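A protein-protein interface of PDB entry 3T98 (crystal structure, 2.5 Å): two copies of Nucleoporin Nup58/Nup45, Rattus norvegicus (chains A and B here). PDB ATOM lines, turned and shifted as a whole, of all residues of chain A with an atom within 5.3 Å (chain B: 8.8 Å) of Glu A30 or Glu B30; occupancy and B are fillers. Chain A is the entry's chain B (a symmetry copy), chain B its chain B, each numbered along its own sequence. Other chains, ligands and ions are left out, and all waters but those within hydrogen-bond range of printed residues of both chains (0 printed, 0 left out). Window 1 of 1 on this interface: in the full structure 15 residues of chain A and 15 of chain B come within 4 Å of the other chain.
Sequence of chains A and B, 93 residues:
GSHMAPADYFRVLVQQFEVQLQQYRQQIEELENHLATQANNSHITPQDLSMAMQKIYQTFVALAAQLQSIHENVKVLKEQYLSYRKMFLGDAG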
ATOM      1  N   ARG A  25      14.923 -16.101  28.568  1.00  0.00           N
ATOM      2  CA  ARG A  25      15.778 -15.604  27.501  1.00  0.00           C
ATOM      3  C   ARG A  25      15.178 -15.808  26.116  1.00  0.00           C
ATOM      4  O   ARG A  25      15.095 -14.869  25.322  1.00  0.00           O
ATOM      5  CB  ARG A  25      17.142 -16.284  27.563  1.00  0.00           C
ATOM      6  CG  ARG A  25      18.065 -15.888  26.435  1.00  0.00           C
ATOM      7  CD  ARG A  25      19.374 -16.633  26.559  1.00  0.00           C
ATOM      8  NE  ARG A  25      20.382 -16.195  25.598  1.00  0.00           N
ATOM      9  CZ  ARG A  25      21.680 -16.467  25.717  1.00  0.00           C
ATOM     10  NH1 ARG A  25      22.115 -17.173  26.754  1.00  0.00           N
ATOM     11  NH2 ARG A  25      22.545 -16.036  24.806  1.00  0.00           N
ATOM     12  N   GLN A  26      14.774 -17.042  25.824  1.00  0.00           N
ATOM     13  CA  GLN A  26      14.186 -17.368  24.528  1.00  0.00           C
ATOM     14  C   GLN A  26      12.954 -16.524  24.255  1.00  0.00           C
ATOM     15  O   GLN A  26      12.847 -15.864  23.218  1.00  0.00           O
ATOM     16  CB  GLN A  26      13.794 -18.841  24.484  1.00  0.00           C
ATOM     17  CG  GLN A  26      14.976 -19.786  24.495  1.00  0.00           C
ATOM     18  CD  GLN A  26      14.550 -21.226  24.671  1.00  0.00           C
ATOM     19  OE1 GLN A  26      15.378 -22.140  24.638  1.00  0.00           O
ATOM     20  NE2 GLN A  26      13.250 -21.438  24.867  1.00  0.00           N
ATOM     21  N   GLN A  27      12.022 -16.564  25.199  1.00  0.00           N
ATOM     22  CA  GLN A  27      10.777 -15.827  25.096  1.00  0.00           C
ATOM     23  C   GLN A  27      10.996 -14.344  24.812  1.00  0.00           C
ATOM     24  O   GLN A  27      10.398 -13.785  23.892  1.00  0.00           O
ATOM     25  CB  GLN A  27       9.982 -15.981  26.390  1.00  0.00           C
ATOM     26  CG  GLN A  27       9.581 -17.400  26.716  1.00  0.00           C
ATOM     27  CD  GLN A  27       8.834 -17.490  28.035  1.00  0.00           C
ATOM     28  OE1 GLN A  27       8.215 -18.506  28.343  1.00  0.00           O
ATOM     29  NE2 GLN A  27       8.895 -16.424  28.827  1.00  0.00           N
ATOM     30  N   ILE A  28      11.845 -13.710  25.611  1.00  0.00           N
ATOM     31  CA  ILE A  28      12.117 -12.293  25.452  1.00  0.00           C
ATOM     32  C   ILE A  28      12.675 -11.995  24.074  1.00  0.00           C
ATOM     33  O   ILE A  28      12.193 -11.089  23.400  1.00  0.00           O
ATOM     34  CB  ILE A  28      13.080 -11.779  26.573  1.00  0.00           C
ATOM     35  CG1 ILE A  28      12.270 -11.045  27.646  1.00  0.00           C
ATOM     36  CG2 ILE A  28      14.118 -10.830  26.011  1.00  0.00           C
ATOM     37  CD1 ILE A  28      11.095 -11.838  28.187  1.00  0.00           C
ATOM     38  N   GLU A  29      13.675 -12.757  23.649  1.00  0.00           N
ATOM     39  CA  GLU A  29      14.263 -12.535  22.339  1.00  0.00           C
ATOM     40  C   GLU A  29      13.179 -12.716  21.284  1.00  0.00           C
ATOM     41  O   GLU A  29      13.101 -11.956  20.317  1.00  0.00           O
ATOM     42  CB  GLU A  29      15.407 -13.523  22.088  1.00  0.00           C
ATOM     43  CG  GLU A  29      16.542 -13.451  23.105  1.00  0.00           C
ATOM     44  CD  GLU A  29      17.729 -14.339  22.733  1.00  0.00           C
ATOM     45  OE1 GLU A  29      17.518 -15.541  22.453  1.00  0.00           O
ATOM     46  OE2 GLU A  29      18.878 -13.837  22.725  1.00  0.00           O
ATOM     47  N   GLU A  30      12.343 -13.730  21.487  1.00  0.00           N
ATOM     48  CA  GLU A  30      11.245 -14.045  20.580  1.00  0.00           C
ATOM     49  C   GLU A  30      10.336 -12.828  20.445  1.00  0.00           C
ATOM     50  O   GLU A  30      10.066 -12.354  19.340  1.00  0.00           O
ATOM     51  CB  GLU A  30      10.436 -15.225  21.138  1.00  0.00           C
ATOM     52  CG  GLU A  30       9.368 -15.783  20.207  1.00  0.00           C
ATOM     53  CD  GLU A  30       9.897 -16.897  19.309  1.00  0.00           C
ATOM     54  OE1 GLU A  30      10.375 -17.919  19.853  1.00  0.00           O
ATOM     55  OE2 GLU A  30       9.835 -16.752  18.065  1.00  0.00           O
ATOM     56  N   LEU A  31       9.870 -12.328  21.584  1.00  0.00           N
ATOM     57  CA  LEU A  31       8.985 -11.179  21.612  1.00  0.00           C
ATOM     58  C   LEU A  31       9.644  -9.906  21.084  1.00  0.00           C
ATOM     59  O   LEU A  31       8.970  -9.051  20.521  1.00  0.00           O
ATOM     60  CB  LEU A  31       8.461 -10.965  23.039  1.00  0.00           C
ATOM     61  CG  LEU A  31       7.412  -9.867  23.258  1.00  0.00           C
ATOM     62  CD1 LEU A  31       6.591  -9.664  22.004  1.00  0.00           C
ATOM     63  CD2 LEU A  31       6.508 -10.246  24.421  1.00  0.00           C
ATOM     64  N   GLU A  32      10.957  -9.781  21.259  1.00  0.00           N
ATOM     65  CA  GLU A  32      11.679  -8.608  20.772  1.00  0.00           C
ATOM     66  C   GLU A  32      11.527  -8.568  19.263  1.00  0.00           C
ATOM     67  O   GLU A  32      11.121  -7.563  18.693  1.00  0.00           O
ATOM     68  CB  GLU A  32      13.174  -8.699  21.110  1.00  0.00           C
ATOM     69  CG  GLU A  32      13.531  -8.675  22.599  1.00  0.00           C
ATOM     70  CD  GLU A  32      13.420  -7.292  23.232  1.00  0.00           C
ATOM     71  OE1 GLU A  32      12.291  -6.754  23.317  1.00  0.00           O
ATOM     72  OE2 GLU A  32      14.469  -6.745  23.643  1.00  0.00           O
ATOM     73  N   ASN A  33      11.858  -9.684  18.627  1.00  0.00           N
ATOM     74  CA  ASN A  33      11.777  -9.810  17.180  1.00  0.00           C
ATOM     75  C   ASN A  33      10.394  -9.515  16.609  1.00  0.00           C
ATOM     76  O   ASN A  33      10.281  -8.895  15.553  1.00  0.00           O
ATOM     77  CB  ASN A  33      12.196 -11.213  16.753  1.00  0.00           C
ATOM     78  CG  ASN A  33      12.025 -11.438  15.269  1.00  0.00           C
ATOM     79  OD1 ASN A  33      12.704 -10.811  14.448  1.00  0.00           O
ATOM     80  ND2 ASN A  33      11.103 -12.327  14.909  1.00  0.00           N
ATOM     81  N   HIS A  34       9.348  -9.967  17.295  1.00  0.00           N
ATOM     82  CA  HIS A  34       7.986  -9.738  16.823  1.00  0.00           C
ATOM     83  C   HIS A  34       7.596  -8.266  16.875  1.00  0.00           C
ATOM     84  O   HIS A  34       6.763  -7.808  16.093  1.00  0.00           O
ATOM     85  CB  HIS A  34       6.979 -10.556  17.638  1.00  0.00           C
ATOM     86  CG  HIS A  34       7.128 -12.034  17.474  1.00  0.00           C
ATOM     87  ND1 HIS A  34       7.598 -12.613  16.311  1.00  0.00           N
ATOM     88  CD2 HIS A  34       6.851 -13.060  18.316  1.00  0.00           C
ATOM     89  CE1 HIS A  34       7.606 -13.926  16.446  1.00  0.00           C
ATOM     90  NE2 HIS A  34       7.157 -14.224  17.654  1.00  0.00           N
ATOM     91  N   GLN B  22       0.594 -20.434  15.895  1.00  0.00           N
ATOM     92  CA  GLN B  22       1.772 -19.600  16.056  1.00  0.00           C
ATOM     93  C   GLN B  22       2.624 -20.131  17.212  1.00  0.00           C
ATOM     94  O   GLN B  22       3.848 -20.233  17.106  1.00  0.00           O
ATOM     95  CB  GLN B  22       1.349 -18.163  16.333  1.00  0.00           C
ATOM     96  CG  GLN B  22       2.513 -17.218  16.345  1.00  0.00           C
ATOM     97  CD  GLN B  22       3.236 -17.175  15.012  1.00  0.00           C
ATOM     98  OE1 GLN B  22       4.428 -16.867  14.956  1.00  0.00           O
ATOM     99  NE2 GLN B  22       2.517 -17.467  13.931  1.00  0.00           N
ATOM    100  N   GLN B  23       1.960 -20.475  18.311  1.00  0.00           N
ATOM    101  CA  GLN B  23       2.619 -21.016  19.501  1.00  0.00           C
ATOM    102  C   GLN B  23       3.502 -22.190  19.095  1.00  0.00           C
ATOM    103  O   GLN B  23       4.725 -22.140  19.221  1.00  0.00           O
ATOM    104  CB  GLN B  23       1.564 -21.515  20.489  1.00  0.00           C
ATOM    105  CG  GLN B  23       2.068 -21.787  21.892  1.00  0.00           C
ATOM    106  CD  GLN B  23       2.307 -20.502  22.655  1.00  0.00           C
ATOM    107  OE1 GLN B  23       3.157 -19.684  22.277  1.00  0.00           O
ATOM    108  NE2 GLN B  23       1.547 -20.304  23.727  1.00  0.00           N
ATOM    109  N   TYR B  24       2.854 -23.249  18.617  1.00  0.00           N
ATOM    110  CA  TYR B  24       3.525 -24.462  18.171  1.00  0.00           C
ATOM    111  C   TYR B  24       4.638 -24.127  17.179  1.00  0.00           C
ATOM    112  O   TYR B  24       5.754 -24.617  17.299  1.00  0.00           O
ATOM    113  CB  TYR B  24       2.512 -25.384  17.496  1.00  0.00           C
ATOM    114  CG  TYR B  24       3.037 -26.761  17.180  1.00  0.00           C
ATOM    115  CD1 TYR B  24       3.104 -27.740  18.166  1.00  0.00           C
ATOM    116  CD2 TYR B  24       3.447 -27.093  15.890  1.00  0.00           C
ATOM    117  CE1 TYR B  24       3.562 -29.024  17.879  1.00  0.00           C
ATOM    118  CE2 TYR B  24       3.910 -28.376  15.585  1.00  0.00           C
ATOM    119  CZ  TYR B  24       3.964 -29.339  16.583  1.00  0.00           C
ATOM    120  OH  TYR B  24       4.397 -30.622  16.292  1.00  0.00           O
ATOM    121  N   ARG B  25       4.323 -23.291  16.199  1.00  0.00           N
ATOM    122  CA  ARG B  25       5.294 -22.902  15.187  1.00  0.00           C
ATOM    123  C   ARG B  25       6.587 -22.361  15.782  1.00  0.00           C
ATOM    124  O   ARG B  25       7.678 -22.810  15.427  1.00  0.00           O
ATOM    125  CB  ARG B  25       4.690 -21.853  14.258  1.00  0.00           C
ATOM    126  CG  ARG B  25       5.661 -21.328  13.228  1.00  0.00           C
ATOM    127  CD  ARG B  25       4.988 -20.274  12.380  1.00  0.00           C
ATOM    128  NE  ARG B  25       5.808 -19.825  11.258  1.00  0.00           N
ATOM    129  CZ  ARG B  25       5.323 -19.157  10.213  1.00  0.00           C
ATOM    130  NH1 ARG B  25       4.028 -18.869  10.155  1.00  0.00           N
ATOM    131  NH2 ARG B  25       6.125 -18.779   9.224  1.00  0.00           N
ATOM    132  N   GLN B  26       6.461 -21.384  16.677  1.00  0.00           N
ATOM    133  CA  GLN B  26       7.626 -20.779  17.316  1.00  0.00           C
ATOM    134  C   GLN B  26       8.454 -21.818  18.049  1.00  0.00           C
ATOM    135  O   GLN B  26       9.662 -21.943  17.832  1.00  0.00           O
ATOM    136  CB  GLN B  26       7.183 -19.711  18.310  1.00  0.00           C
ATOM    137  CG  GLN B  26       6.562 -18.493  17.662  1.00  0.00           C
ATOM    138  CD  GLN B  26       5.941 -17.562  18.677  1.00  0.00           C
ATOM    139  OE1 GLN B  26       5.446 -16.486  18.331  1.00  0.00           O
ATOM    140  NE2 GLN B  26       5.958 -17.973  19.944  1.00  0.00           N
ATOM    141  N   GLN B  27       7.786 -22.555  18.927  1.00  0.00           N
ATOM    142  CA  GLN B  27       8.425 -23.587  19.722  1.00  0.00           C
ATOM    143  C   GLN B  27       9.202 -24.586  18.871  1.00  0.00           C
ATOM    144  O   GLN B  27      10.369 -24.868  19.141  1.00  0.00           O
ATOM    145  CB  GLN B  27       7.369 -24.332  20.536  1.00  0.00           C
ATOM    146  CG  GLN B  27       6.616 -23.473  21.525  1.00  0.00           C
ATOM    147  CD  GLN B  27       5.553 -24.262  22.268  1.00  0.00           C
ATOM    148  OE1 GLN B  27       5.018 -23.808  23.276  1.00  0.00           O
ATOM    149  NE2 GLN B  27       5.237 -25.452  21.767  1.00  0.00           N
ATOM    150  N   ILE B  28       8.548 -25.125  17.850  1.00  0.00           N
ATOM    151  CA  ILE B  28       9.176 -26.105  16.982  1.00  0.00           C
ATOM    152  C   ILE B  28      10.412 -25.532  16.317  1.00  0.00           C
ATOM    153  O   ILE B  28      11.468 -26.159  16.338  1.00  0.00           O
ATOM    154  CB  ILE B  28       8.163 -26.644  15.920  1.00  0.00           C
ATOM    155  CG1 ILE B  28       7.650 -28.020  16.353  1.00  0.00           C
ATOM    156  CG2 ILE B  28       8.813 -26.773  14.558  1.00  0.00           C
ATOM    157  CD1 ILE B  28       7.107 -28.062  17.770  1.00  0.00           C
ATOM    158  N   GLU B  29      10.292 -24.343  15.740  1.00  0.00           N
ATOM    159  CA  GLU B  29      11.431 -23.725  15.083  1.00  0.00           C
ATOM    160  C   GLU B  29      12.539 -23.533  16.110  1.00  0.00           C
ATOM    161  O   GLU B  29      13.716 -23.759  15.825  1.00  0.00           O
ATOM    162  CB  GLU B  29      11.037 -22.373  14.479  1.00  0.00           C
ATOM    163  CG  GLU B  29       9.911 -22.441  13.452  1.00  0.00           C
ATOM    164  CD  GLU B  29       9.655 -21.101  12.763  1.00  0.00           C
ATOM    165  OE1 GLU B  29       9.490 -20.081  13.471  1.00  0.00           O
ATOM    166  OE2 GLU B  29       9.612 -21.065  11.511  1.00  0.00           O
ATOM    167  N   GLU B  30      12.143 -23.117  17.310  1.00  0.00           N
ATOM    168  CA  GLU B  30      13.070 -22.886  18.413  1.00  0.00           C
ATOM    169  C   GLU B  30      13.849 -24.165  18.696  1.00  0.00           C
ATOM    170  O   GLU B  30      15.081 -24.172  18.704  1.00  0.00           O
ATOM    171  CB  GLU B  30      12.286 -22.479  19.669  1.00  0.00           C
ATOM    172  CG  GLU B  30      13.135 -22.028  20.851  1.00  0.00           C
ATOM    173  CD  GLU B  30      13.403 -20.526  20.839  1.00  0.00           C
ATOM    174  OE1 GLU B  30      12.421 -19.749  20.869  1.00  0.00           O
ATOM    175  OE2 GLU B  30      14.590 -20.125  20.802  1.00  0.00           O
ATOM    176  N   LEU B  31      13.115 -25.248  18.923  1.00  0.00           N
ATOM    177  CA  LEU B  31      13.717 -26.536  19.219  1.00  0.00           C
ATOM    178  C   LEU B  31      14.541 -27.087  18.057  1.00  0.00           C
ATOM    179  O   LEU B  31      15.516 -27.795  18.276  1.00  0.00           O
ATOM    180  CB  LEU B  31      12.626 -27.533  19.631  1.00  0.00           C
ATOM    181  CG  LEU B  31      13.071 -28.925  20.100  1.00  0.00           C
ATOM    182  CD1 LEU B  31      14.449 -28.857  20.719  1.00  0.00           C
ATOM    183  CD2 LEU B  31      12.071 -29.471  21.107  1.00  0.00           C
ATOM    184  N   GLU B  32      14.154 -26.762  16.826  1.00  0.00           N
ATOM    185  CA  GLU B  32      14.890 -27.227  15.653  1.00  0.00           C
ATOM    186  C   GLU B  32      16.294 -26.659  15.735  1.00  0.00           C
ATOM    187  O   GLU B  32      17.278 -27.384  15.647  1.00  0.00           O
ATOM    188  CB  GLU B  32      14.236 -26.728  14.356  1.00  0.00           C
ATOM    189  CG  GLU B  32      12.832 -27.261  14.061  1.00  0.00           C
ATOM    190  CD  GLU B  32      12.816 -28.705  13.573  1.00  0.00           C
ATOM    191  OE1 GLU B  32      13.183 -29.613  14.355  1.00  0.00           O
ATOM    192  OE2 GLU B  32      12.434 -28.928  12.400  1.00  0.00           O
ATOM    193  N   ASN B  33      16.368 -25.346  15.909  1.00  0.00           N
ATOM    194  CA  ASN B  33      17.638 -24.643  16.001  1.00  0.00           C
ATOM    195  C   ASN B  33      18.556 -25.164  17.102  1.00  0.00           C
ATOM    196  O   ASN B  33      19.767 -25.250  16.907  1.00  0.00           O
ATOM    197  CB  ASN B  33      17.396 -23.153  16.227  1.00  0.00           C
ATOM    198  CG  ASN B  33      18.681 -22.388  16.443  1.00  0.00           C
ATOM    199  OD1 ASN B  33      19.516 -22.280  15.538  1.00  0.00           O
ATOM    200  ND2 ASN B  33      18.858 -21.861  17.651  1.00  0.00           N
ATOM    201  N   HIS B  34      17.987 -25.496  18.257  1.00  0.00           N
ATOM    202  CA  HIS B  34      18.786 -25.999  19.370  1.00  0.00           C
ATOM    203  C   HIS B  34      19.386 -27.369  19.079  1.00  0.00           C
ATOM    204  O   HIS B  34      20.440 -27.720  19.609  1.00  0.00           O
ATOM    205  CB  HIS B  34      17.952 -26.075  20.652  1.00  0.00           C
ATOM    206  CG  HIS B  34      17.501 -24.743  21.160  1.00  0.00           C
ATOM    207  ND1 HIS B  34      18.225 -23.584  20.962  1.00  0.00           N
ATOM    208  CD2 HIS B  34      16.409 -24.382  21.878  1.00  0.00           C
ATOM    209  CE1 HIS B  34      17.599 -22.572  21.532  1.00  0.00           C
ATOM    210  NE2 HIS B  34      16.494 -23.029  22.095  1.00  0.00           N
ATOM    211  N   LEU B  35      18.716 -28.141  18.232  1.00  0.00           N
ATOM    212  CA  LEU B  35      19.200 -29.464  17.884  1.00  0.00           C
ATOM    213  C   LEU B  35      19.817 -29.476  16.495  1.00  0.00           C
ATOM    214  O   LEU B  35      20.221 -30.527  15.998  1.00  0.00           O
ATOM    215  CB  LEU B  35      18.056 -30.480  17.963  1.00  0.00           C
ATOM    216  CG  LEU B  35      17.403 -30.606  19.343  1.00  0.00           C
ATOM    217  CD1 LEU B  35      16.467 -31.803  19.372  1.00  0.00           C
ATOM    218  CD2 LEU B  35      18.481 -30.763  20.407  1.00  0.00           C
ATOM    219  N   ALA B  36      19.898 -28.303  15.876  1.00  0.00           N
ATOM    220  CA  ALA B  36      20.465 -28.181  14.534  1.00  0.00           C
ATOM    221  C   ALA B  36      21.930 -28.610  14.492  1.00  0.00           C
ATOM    222  O   ALA B  36      22.392 -29.193  13.507  1.00  0.00           O
ATOM    223  CB  ALA B  36      20.327 -26.749  14.040  1.00  0.00           C
ATOM    224  N   ASN B  40      25.235 -25.361  18.778  1.00  0.00           N
ATOM    225  CA  ASN B  40      24.093 -24.654  19.342  1.00  0.00           C
ATOM    226  C   ASN B  40      23.536 -25.437  20.518  1.00  0.00           C
ATOM    227  O   ASN B  40      22.930 -24.871  21.429  1.00  0.00           O
ATOM    228  CB  ASN B  40      22.999 -24.491  18.287  1.00  0.00           C
ATOM    229  CG  ASN B  40      23.547 -24.060  16.942  1.00  0.00           C
ATOM    230  OD1 ASN B  40      24.447 -23.220  16.865  1.00  0.00           O
ATOM    231  ND2 ASN B  40      22.999 -24.626  15.872  1.00  0.00           N
ATOM    232  N   ILE B  44      22.625 -25.047  25.510  1.00  0.00           N
ATOM    233  CA  ILE B  44      21.417 -25.529  26.169  1.00  0.00           C
ATOM    234  C   ILE B  44      21.757 -26.758  27.013  1.00  0.00           C
ATOM    235  O   ILE B  44      22.816 -27.350  26.857  1.00  0.00           O
ATOM    236  CB  ILE B  44      20.338 -25.924  25.124  1.00  0.00           C
ATOM    237  CG1 ILE B  44      18.948 -25.867  25.750  1.00  0.00           C
ATOM    238  CG2 ILE B  44      20.584 -27.338  24.610  1.00  0.00           C
ATOM    239  CD1 ILE B  44      18.462 -24.468  26.003  1.00  0.00           C
ATOM    240  N   LEU B  49      15.804 -28.958  27.055  1.00  0.00           N
ATOM    241  CA  LEU B  49      15.135 -29.714  26.009  1.00  0.00           C
ATOM    242  C   LEU B  49      13.962 -30.402  26.683  1.00  0.00           C
ATOM    243  O   LEU B  49      12.846 -30.374  26.183  1.00  0.00           O
ATOM    244  CB  LEU B  49      16.072 -30.764  25.426  1.00  0.00           C
ATOM    245  CG  LEU B  49      17.284 -30.266  24.641  1.00  0.00           C
ATOM    246  CD1 LEU B  49      18.181 -31.454  24.304  1.00  0.00           C
ATOM    247  CD2 LEU B  49      16.836 -29.564  23.376  1.00  0.00           C
ATOM    248  N   ALA B  52      11.295 -27.886  26.956  1.00  0.00           N
ATOM    249  CA  ALA B  52      10.720 -27.598  25.653  1.00  0.00           C
ATOM    250  C   ALA B  52       9.832 -28.748  25.152  1.00  0.00           C
ATOM    251  O   ALA B  52       8.721 -28.514  24.672  1.00  0.00           O
ATOM    252  CB  ALA B  52      11.845 -27.306  24.645  1.00  0.00           C
ATOM    253  N   ILE B  56       6.129 -28.047  24.035  1.00  0.00           N
ATOM    254  CA  ILE B  56       5.705 -28.434  22.697  1.00  0.00           C
ATOM    255  C   ILE B  56       4.584 -29.468  22.668  1.00  0.00           C
ATOM    256  O   ILE B  56       3.637 -29.329  21.909  1.00  0.00           O
ATOM    257  CB  ILE B  56       6.893 -28.962  21.879  1.00  0.00           C
ATOM    258  CG1 ILE B  56       7.883 -27.823  21.641  1.00  0.00           C
ATOM    259  CG2 ILE B  56       6.411 -29.534  20.562  1.00  0.00           C
ATOM    260  CD1 ILE B  56       9.146 -28.227  20.902  1.00  0.00           C
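A ring nitrogen (NE2) of His B34 lies within hydrogen-bond range of the side-chain amide oxygen (OE1) of Gln A26 (2.9 Å). The side-chain carboxylate (OE1) of Glu A30 lies close to the side-chain carboxylate (OE1) of Glu B30, 2.9 Å away. A ring nitrogen (NE2) of His A34 lies within hydrogen-bond range of the side-chain amide oxygen (OE1) of Gln B26 (2.9 Å).
Among the printed residues, merely in contact across the chains: Gln A26 with Glu B30 (3.7 Å) and Glu A30 with Gln B26 (3.7 Å).
Glu A30 touches two residues of chain B. Printed residues of chain A within 4 Å of Glu B30: Gln A26 and Glu A30. Of the printed residues of chain B, Gln A26 touches Glu B30 (3.7 Å) and His B34 (2.9 Å). Of the printed residues of chain A, Gln B26 touches Glu A30 (3.7 Å) and His A34 (2.9 Å). Printed residues of chain A within 4 Å of His B34: Gln A26. Of the printed residues of chain B, His A34 touches Gln B26 (2.9 Å). The nearest printed residue of chain B that does not touch His A34 is Gln B22 (4.6 Å).
Hydrophobic or aromatic side chains of chain B within 4 Å of the printed part of chain A: His B34. Printed residues of chain A that touch a printed residue of chain B: Gln A26, Glu A30 and His A34.
Gln A26 touches Glu B30, and with the chains exchanged Glu A30 touches Gln B26. Gln A26 touches His B34, and with the chains exchanged His A34 touches Gln B26. Glu A30 touches its own counterpart, Glu B30. Positions printed for both chains: 25, 26, 27, 28, 29, 30, 31, 32, 33 and 34. Of the 5 pairs that touch across the chains among the printed residues, 5 have their exchanged pair printed and touching as well.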
